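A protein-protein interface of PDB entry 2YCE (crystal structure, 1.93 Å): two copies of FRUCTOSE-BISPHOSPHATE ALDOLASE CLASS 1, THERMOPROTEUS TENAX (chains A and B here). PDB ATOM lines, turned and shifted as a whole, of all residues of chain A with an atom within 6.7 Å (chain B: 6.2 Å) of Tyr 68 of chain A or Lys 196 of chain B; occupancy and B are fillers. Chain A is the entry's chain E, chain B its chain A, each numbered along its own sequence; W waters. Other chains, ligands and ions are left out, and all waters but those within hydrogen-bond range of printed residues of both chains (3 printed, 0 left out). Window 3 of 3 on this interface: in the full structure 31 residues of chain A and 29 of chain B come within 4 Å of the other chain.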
ATOM      1  N   ALA A  41     -19.912 -22.981  16.587  1.00  0.00           N
ATOM      2  CA  ALA A  41     -19.740 -22.673  15.143  1.00  0.00           C
ATOM      3  C   ALA A  41     -19.003 -23.797  14.384  1.00  0.00           C
ATOM      4  O   ALA A  41     -19.038 -23.866  13.149  1.00  0.00           O
ATOM      5  CB  ALA A  41     -18.987 -21.326  14.956  1.00  0.00           C
ATOM      6  N   ASP A  42     -18.342 -24.668  15.134  1.00  0.00           N
ATOM      7  CA  ASP A  42     -17.573 -25.771  14.582  1.00  0.00           C
ATOM      8  C   ASP A  42     -18.409 -27.070  14.523  1.00  0.00           C
ATOM      9  O   ASP A  42     -18.727 -27.638  15.587  1.00  0.00           O
ATOM     10  CB  ASP A  42     -16.291 -25.972  15.450  1.00  0.00           C
ATOM     11  CG  ASP A  42     -15.436 -27.132  14.979  1.00  0.00           C
ATOM     12  OD1 ASP A  42     -15.760 -27.779  13.946  1.00  0.00           O
ATOM     13  OD2 ASP A  42     -14.404 -27.374  15.616  1.00  0.00           O
ATOM     14  N   PRO A  43     -18.775 -27.551  13.296  1.00  0.00           N
ATOM     15  CA  PRO A  43     -19.629 -28.756  13.222  1.00  0.00           C
ATOM     16  C   PRO A  43     -18.943 -29.955  13.859  1.00  0.00           C
ATOM     17  O   PRO A  43     -19.643 -30.860  14.309  1.00  0.00           O
ATOM     18  CB  PRO A  43     -19.821 -28.981  11.716  1.00  0.00           C
ATOM     19  CG  PRO A  43     -19.644 -27.612  11.117  1.00  0.00           C
ATOM     20  CD  PRO A  43     -18.524 -26.990  11.952  1.00  0.00           C
ATOM     21  N   GLU A  44     -17.606 -29.977  13.894  1.00  0.00           N
ATOM     22  CA  GLU A  44     -16.900 -31.078  14.576  1.00  0.00           C
ATOM     23  C   GLU A  44     -17.211 -31.138  16.074  1.00  0.00           C
ATOM     24  O   GLU A  44     -17.337 -32.232  16.642  1.00  0.00           O
ATOM     25  CB  GLU A  44     -15.374 -31.016  14.372  1.00  0.00           C
ATOM     26  CG  GLU A  44     -14.924 -31.666  13.066  1.00  0.00           C
ATOM     27  CD  GLU A  44     -13.464 -31.335  12.683  1.00  0.00           C
ATOM     28  OE1 GLU A  44     -12.580 -31.386  13.545  1.00  0.00           O
ATOM     29  OE2 GLU A  44     -13.205 -31.003  11.508  1.00  0.00           O
ATOM     30  N   LEU A  47     -20.776 -32.658  16.371  1.00  0.00           N
ATOM     31  CA  LEU A  47     -20.641 -34.122  16.305  1.00  0.00           C
ATOM     32  C   LEU A  47     -20.148 -34.775  17.604  1.00  0.00           C
ATOM     33  O   LEU A  47     -20.732 -35.771  18.043  1.00  0.00           O
ATOM     34  CB  LEU A  47     -19.767 -34.548  15.129  1.00  0.00           C
ATOM     35  CG  LEU A  47     -20.436 -34.419  13.754  1.00  0.00           C
ATOM     36  CD1 LEU A  47     -19.409 -34.636  12.666  1.00  0.00           C
ATOM     37  CD2 LEU A  47     -21.596 -35.434  13.598  1.00  0.00           C
ATOM     38  N   PHE A  60     -28.239 -31.835   9.853  1.00  0.00           N
ATOM     39  CA  PHE A  60     -27.329 -30.955   9.097  1.00  0.00           C
ATOM     40  C   PHE A  60     -27.954 -30.613   7.752  1.00  0.00           C
ATOM     41  O   PHE A  60     -28.667 -31.444   7.169  1.00  0.00           O
ATOM     42  CB  PHE A  60     -26.030 -31.686   8.702  1.00  0.00           C
ATOM     43  CG  PHE A  60     -25.033 -31.922   9.829  1.00  0.00           C
ATOM     44  CD1 PHE A  60     -25.101 -31.226  11.052  1.00  0.00           C
ATOM     45  CD2 PHE A  60     -23.979 -32.828   9.617  1.00  0.00           C
ATOM     46  CE1 PHE A  60     -24.143 -31.458  12.055  1.00  0.00           C
ATOM     47  CE2 PHE A  60     -23.018 -33.072  10.594  1.00  0.00           C
ATOM     48  CZ  PHE A  60     -23.097 -32.378  11.828  1.00  0.00           C
ATOM     49  N   GLY A  63     -24.355 -28.847   3.020  1.00  0.00           N
ATOM     50  CA  GLY A  63     -22.953 -28.419   2.974  1.00  0.00           C
ATOM     51  C   GLY A  63     -22.198 -28.825   4.231  1.00  0.00           C
ATOM     52  O   GLY A  63     -21.040 -29.201   4.176  1.00  0.00           O
ATOM     53  N   ILE A  64     -22.880 -28.762   5.364  1.00  0.00           N
ATOM     54  CA  ILE A  64     -22.315 -29.285   6.598  1.00  0.00           C
ATOM     55  C   ILE A  64     -22.142 -30.822   6.571  1.00  0.00           C
ATOM     56  O   ILE A  64     -21.132 -31.326   7.002  1.00  0.00           O
ATOM     57  CB  ILE A  64     -23.129 -28.850   7.846  1.00  0.00           C
ATOM     58  CG1 ILE A  64     -23.274 -27.307   7.896  1.00  0.00           C
ATOM     59  CG2 ILE A  64     -22.449 -29.413   9.117  1.00  0.00           C
ATOM     60  CD1 ILE A  64     -21.985 -26.522   8.220  1.00  0.00           C
ATOM     61  N   ALA A  65     -23.130 -31.564   6.088  1.00  0.00           N
ATOM     62  CA  ALA A  65     -22.970 -33.023   5.943  1.00  0.00           C
ATOM     63  C   ALA A  65     -21.789 -33.336   5.007  1.00  0.00           C
ATOM     64  O   ALA A  65     -20.951 -34.196   5.300  1.00  0.00           O
ATOM     65  CB  ALA A  65     -24.279 -33.673   5.425  1.00  0.00           C
ATOM     66  N   GLU A  66     -21.698 -32.610   3.892  1.00  0.00           N
ATOM     67  CA  GLU A  66     -20.685 -32.958   2.905  1.00  0.00           C
ATOM     68  C   GLU A  66     -19.302 -32.764   3.468  1.00  0.00           C
ATOM     69  O   GLU A  66     -18.467 -33.629   3.327  1.00  0.00           O
ATOM     70  CB  GLU A  66     -20.834 -32.169   1.612  1.00  0.00           C
ATOM     71  CG  GLU A  66     -19.828 -32.559   0.535  1.00  0.00           C
ATOM     72  CD  GLU A  66     -20.006 -31.649  -0.669  1.00  0.00           C
ATOM     73  OE1 GLU A  66     -19.574 -30.487  -0.606  1.00  0.00           O
ATOM     74  OE2 GLU A  66     -20.643 -32.077  -1.652  1.00  0.00           O
ATOM     75  N   LYS A  67     -19.073 -31.617   4.101  1.00  0.00           N
ATOM     76  CA  LYS A  67     -17.721 -31.269   4.548  1.00  0.00           C
ATOM     77  C   LYS A  67     -17.343 -31.890   5.898  1.00  0.00           C
ATOM     78  O   LYS A  67     -16.152 -32.041   6.200  1.00  0.00           O
ATOM     79  CB  LYS A  67     -17.590 -29.747   4.617  1.00  0.00           C
ATOM     80  CG  LYS A  67     -16.965 -29.143   3.381  1.00  0.00           C
ATOM     81  CD  LYS A  67     -17.907 -29.123   2.238  1.00  0.00           C
ATOM     82  CE  LYS A  67     -17.276 -28.376   1.036  1.00  0.00           C
ATOM     83  NZ  LYS A  67     -18.394 -28.266   0.022  1.00  0.00           N
ATOM     84  N   TYR A  68     -18.345 -32.273   6.699  1.00  0.00           N
ATOM     85  CA  TYR A  68     -18.048 -32.678   8.087  1.00  0.00           C
ATOM     86  C   TYR A  68     -18.570 -34.047   8.517  1.00  0.00           C
ATOM     87  O   TYR A  68     -18.015 -34.641   9.433  1.00  0.00           O
ATOM     88  CB  TYR A  68     -18.578 -31.623   9.059  1.00  0.00           C
ATOM     89  CG  TYR A  68     -17.821 -30.311   8.971  1.00  0.00           C
ATOM     90  CD1 TYR A  68     -16.692 -30.071   9.773  1.00  0.00           C
ATOM     91  CD2 TYR A  68     -18.241 -29.301   8.089  1.00  0.00           C
ATOM     92  CE1 TYR A  68     -15.996 -28.880   9.695  1.00  0.00           C
ATOM     93  CE2 TYR A  68     -17.538 -28.081   8.007  1.00  0.00           C
ATOM     94  CZ  TYR A  68     -16.429 -27.886   8.808  1.00  0.00           C
ATOM     95  OH  TYR A  68     -15.749 -26.692   8.740  1.00  0.00           O
ATOM     96  N   TYR A  69     -19.647 -34.539   7.898  1.00  0.00           N
ATOM     97  CA  TYR A  69     -20.277 -35.727   8.454  1.00  0.00           C
ATOM     98  C   TYR A  69     -19.351 -36.932   8.381  1.00  0.00           C
ATOM     99  O   TYR A  69     -18.729 -37.174   7.338  1.00  0.00           O
ATOM    100  CB  TYR A  69     -21.623 -36.042   7.788  1.00  0.00           C
ATOM    101  CG  TYR A  69     -22.304 -37.247   8.420  1.00  0.00           C
ATOM    102  CD1 TYR A  69     -22.706 -37.218   9.771  1.00  0.00           C
ATOM    103  CD2 TYR A  69     -22.554 -38.407   7.683  1.00  0.00           C
ATOM    104  CE1 TYR A  69     -23.340 -38.323  10.376  1.00  0.00           C
ATOM    105  CE2 TYR A  69     -23.198 -39.527   8.283  1.00  0.00           C
ATOM    106  CZ  TYR A  69     -23.593 -39.464   9.623  1.00  0.00           C
ATOM    107  OH  TYR A  69     -24.223 -40.544  10.211  1.00  0.00           O
ATOM    108  N   ASP A  70     -19.237 -37.669   9.489  1.00  0.00           N
ATOM    109  CA  ASP A  70     -18.246 -38.766   9.595  1.00  0.00           C
ATOM    110  C   ASP A  70     -18.852 -40.141   9.912  1.00  0.00           C
ATOM    111  O   ASP A  70     -18.127 -41.070  10.254  1.00  0.00           O
ATOM    112  CB  ASP A  70     -17.163 -38.420  10.663  1.00  0.00           C
ATOM    113  CG  ASP A  70     -17.765 -38.227  12.082  1.00  0.00           C
ATOM    114  OD1 ASP A  70     -19.009 -38.333  12.287  1.00  0.00           O
ATOM    115  OD2 ASP A  70     -16.997 -37.946  13.004  1.00  0.00           O
ATOM    116  N   GLY A  71     -20.172 -40.270   9.802  1.00  0.00           N
ATOM    117  CA  GLY A  71     -20.854 -41.529  10.103  1.00  0.00           C
ATOM    118  C   GLY A  71     -21.003 -41.866  11.583  1.00  0.00           C
ATOM    119  O   GLY A  71     -21.522 -42.925  11.899  1.00  0.00           O
ATOM    120  N   THR B   5     -12.920 -28.830  -2.800  1.00  0.00           N
ATOM    121  CA  THR B   5     -12.168 -27.750  -2.153  1.00  0.00           C
ATOM    122  C   THR B   5     -10.653 -27.965  -2.368  1.00  0.00           C
ATOM    123  O   THR B   5      -9.932 -27.012  -2.705  1.00  0.00           O
ATOM    124  CB  THR B   5     -12.502 -27.631  -0.643  1.00  0.00           C
ATOM    125  OG1 THR B   5     -13.851 -27.184  -0.495  1.00  0.00           O
ATOM    126  CG2 THR B   5     -11.550 -26.645   0.075  1.00  0.00           C
ATOM    127  N   LEU B 169     -21.254 -21.884   3.138  1.00  0.00           N
ATOM    128  CA  LEU B 169     -20.830 -23.181   3.646  1.00  0.00           C
ATOM    129  C   LEU B 169     -22.045 -24.142   3.698  1.00  0.00           C
ATOM    130  O   LEU B 169     -21.980 -25.295   3.201  1.00  0.00           O
ATOM    131  CB  LEU B 169     -20.200 -23.030   5.023  1.00  0.00           C
ATOM    132  CG  LEU B 169     -20.024 -24.317   5.845  1.00  0.00           C
ATOM    133  CD1 LEU B 169     -19.099 -25.315   5.155  1.00  0.00           C
ATOM    134  CD2 LEU B 169     -19.575 -24.036   7.293  1.00  0.00           C
ATOM    135  N   ASP B 174     -17.655 -24.966  -2.491  1.00  0.00           N
ATOM    136  CA  ASP B 174     -16.289 -25.454  -2.316  1.00  0.00           C
ATOM    137  C   ASP B 174     -15.284 -24.317  -2.009  1.00  0.00           C
ATOM    138  O   ASP B 174     -14.246 -24.564  -1.400  1.00  0.00           O
ATOM    139  CB  ASP B 174     -15.877 -26.311  -3.520  1.00  0.00           C
ATOM    140  CG  ASP B 174     -16.889 -27.434  -3.789  1.00  0.00           C
ATOM    141  OD1 ASP B 174     -17.179 -28.186  -2.817  1.00  0.00           O
ATOM    142  OD2 ASP B 174     -17.423 -27.526  -4.934  1.00  0.00           O
ATOM    143  N   LYS B 192     -13.866 -17.788  10.205  1.00  0.00           N
ATOM    144  CA  LYS B 192     -14.032 -18.949  11.097  1.00  0.00           C
ATOM    145  C   LYS B 192     -15.360 -19.713  10.844  1.00  0.00           C
ATOM    146  O   LYS B 192     -15.373 -20.947  10.830  1.00  0.00           O
ATOM    147  CB  LYS B 192     -13.936 -18.480  12.559  1.00  0.00           C
ATOM    148  CG  LYS B 192     -14.323 -19.499  13.652  1.00  0.00           C
ATOM    149  CD  LYS B 192     -13.355 -20.677  13.831  1.00  0.00           C
ATOM    150  CE  LYS B 192     -13.164 -21.046  15.340  1.00  0.00           C
ATOM    151  NZ  LYS B 192     -14.321 -20.631  16.238  1.00  0.00           N
ATOM    152  N   ALA B 194     -17.039 -19.961   8.171  1.00  0.00           N
ATOM    153  CA  ALA B 194     -16.952 -20.674   6.873  1.00  0.00           C
ATOM    154  C   ALA B 194     -16.272 -22.052   7.010  1.00  0.00           C
ATOM    155  O   ALA B 194     -16.301 -22.859   6.061  1.00  0.00           O
ATOM    156  CB  ALA B 194     -16.222 -19.835   5.821  1.00  0.00           C
ATOM    157  N   GLY B 195     -15.640 -22.301   8.156  1.00  0.00           N
ATOM    158  CA  GLY B 195     -15.051 -23.609   8.425  1.00  0.00           C
ATOM    159  C   GLY B 195     -13.978 -23.992   7.414  1.00  0.00           C
ATOM    160  O   GLY B 195     -13.059 -23.194   7.140  1.00  0.00           O
ATOM    161  N   LYS B 196     -14.108 -25.206   6.855  1.00  0.00           N
ATOM    162  CA  LYS B 196     -13.171 -25.794   5.868  1.00  0.00           C
ATOM    163  C   LYS B 196     -13.233 -25.129   4.487  1.00  0.00           C
ATOM    164  O   LYS B 196     -12.431 -25.457   3.613  1.00  0.00           O
ATOM    165  CB  LYS B 196     -13.496 -27.288   5.660  1.00  0.00           C
ATOM    166  CG  LYS B 196     -13.110 -28.189   6.800  1.00  0.00           C
ATOM    167  CD  LYS B 196     -13.410 -29.638   6.403  1.00  0.00           C
ATOM    168  CE  LYS B 196     -13.332 -30.480   7.633  1.00  0.00           C
ATOM    169  NZ  LYS B 196     -13.643 -31.899   7.306  1.00  0.00           N
ATOM    170  N   VAL B 197     -14.221 -24.266   4.261  1.00  0.00           N
ATOM    171  CA  VAL B 197     -14.365 -23.623   2.952  1.00  0.00           C
ATOM    172  C   VAL B 197     -13.561 -22.319   2.846  1.00  0.00           C
ATOM    173  O   VAL B 197     -13.767 -21.411   3.641  1.00  0.00           O
ATOM    174  CB  VAL B 197     -15.857 -23.389   2.576  1.00  0.00           C
ATOM    175  CG1 VAL B 197     -15.960 -22.592   1.252  1.00  0.00           C
ATOM    176  CG2 VAL B 197     -16.525 -24.748   2.440  1.00  0.00           C
ATOM    177  N   PRO B 198     -12.637 -22.228   1.863  1.00  0.00           N
ATOM    178  CA  PRO B 198     -11.798 -21.014   1.795  1.00  0.00           C
ATOM    179  C   PRO B 198     -12.589 -19.770   1.395  1.00  0.00           C
ATOM    180  O   PRO B 198     -13.595 -19.854   0.666  1.00  0.00           O
ATOM    181  CB  PRO B 198     -10.696 -21.376   0.783  1.00  0.00           C
ATOM    182  CG  PRO B 198     -11.299 -22.482  -0.040  1.00  0.00           C
ATOM    183  CD  PRO B 198     -12.233 -23.243   0.877  1.00  0.00           C
HETATM  184  O   HOH W   1     -16.444 -23.238  11.994  1.00  0.00           O
HETATM  185  O   HOH W   2     -13.981 -32.905   9.721  1.00  0.00           O
HETATM  186  O   HOH W   3     -19.973 -26.573   1.619  1.00  0.00           O
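Water W2 bridges NZ of Lys 196 of chain B (2.6 Å) and OE2 of Glu 44 of chain A (2.7 Å). Water W1 bridges O of Lys 192 of chain B (2.8 Å) and O of Ala 41 of chain A (2.9 Å). Water W3 bridges NZ of Lys 67 of chain A and O of Leu 169 of chain B.
No position is printed for both chains. Of the 10 pairs that touch across the chains among the printed residues, none has its exchanged pair printed and touching as well.
The side-chain amino group of Lys 67 of chain A is in salt-bridge range of the side-chain carboxylate of Glu 66 of chain A, at 2.6 Å. The side-chain carboxylate (OD1) of Asp 42 of chain A lies within hydrogen-bond range of the backbone NH (N) of Glu 44 of chain A, at 2.9 Å. O of Asp 174 of chain B sits at hydrogen-bond distance from OG1 of Thr 5 of chain B (2.8 Å).
NZ of Lys 196 of chain B is in hydrogen-bond range of O of Lys 67 of chain A (2.7 Å). The backbone NH of Lys 196 of chain B lies within hydrogen-bond range of the side-chain hydroxyl of Tyr 68 of chain A (2.9 Å). The side-chain amino group of Lys 67 of chain A lies within salt-bridge range of the side-chain carboxylate of Asp 174 of chain B (3.1 Å).
Of chain A, only Glu 44 (3.9 Å), Lys 67 (2.7 Å) and Tyr 68 (2.9 Å) come within 4 Å of Lys 196 of chain B. Of the printed residues of chain B, Glu 44 of chain A touches Lys 196 (3.9 Å). Of the printed residues of chain A, Thr 5 of chain B touches Lys 67. Printed residues of chain B within 4 Å of Lys 67 of chain A: Thr 5, Asp 174, Lys 196 and Val 197. Of the printed residues of chain A, Leu 169 of chain B touches Gly 63 (3.3 Å) and Ile 64 (3.6 Å). Of the printed residues of chain A, Val 197 of chain B touches Lys 67 (3.96 Å). Lys 192 of chain B touches none of the printed residues of chain A. Ala 41 of chain A touches none of the printed residues of chain B. The nearest residue of chain A that does not touch Lys 196 of chain B is Glu 66 of chain A (6.5 Å). The nearest printed residue of chain B that does not touch Lys 67 of chain A is Leu 169 of chain B (4.7 Å).
Lys 196 of chain B touches Glu 44 of chain A (CE to OE2, 3.9 Å). CA of Gly 63 of chain A touches O of Leu 169 of chain B, at 3.3 Å. CD1 of Ile 64 of chain A touches CD2 of Leu 169 of chain B (3.6 Å). OE1 of Glu 66 of chain A touches OD1 of Asp 174 of chain B, 3.99 Å away. Thr 5 of chain B touches Lys 67 of chain A (OG1 to CE, 3.9 Å). CE of Lys 67 of chain A touches CG2 of Val 197 of chain B, at 3.96 Å. Tyr 68 of chain A touches Gly 195 of chain B.
Of the 15 printed residues of chain A, 6 touch a printed residue of chain B. Printed residues of chain A that touch a printed residue of chain B: Glu 44, Gly 63, Ile 64, Glu 66, Lys 67 and Tyr 68. Hydrophobic or aromatic side chains of chain B that line the printed part of chain A: Leu 169 and Val 197. Among the printed residues, 10 pairs touch across the chains.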
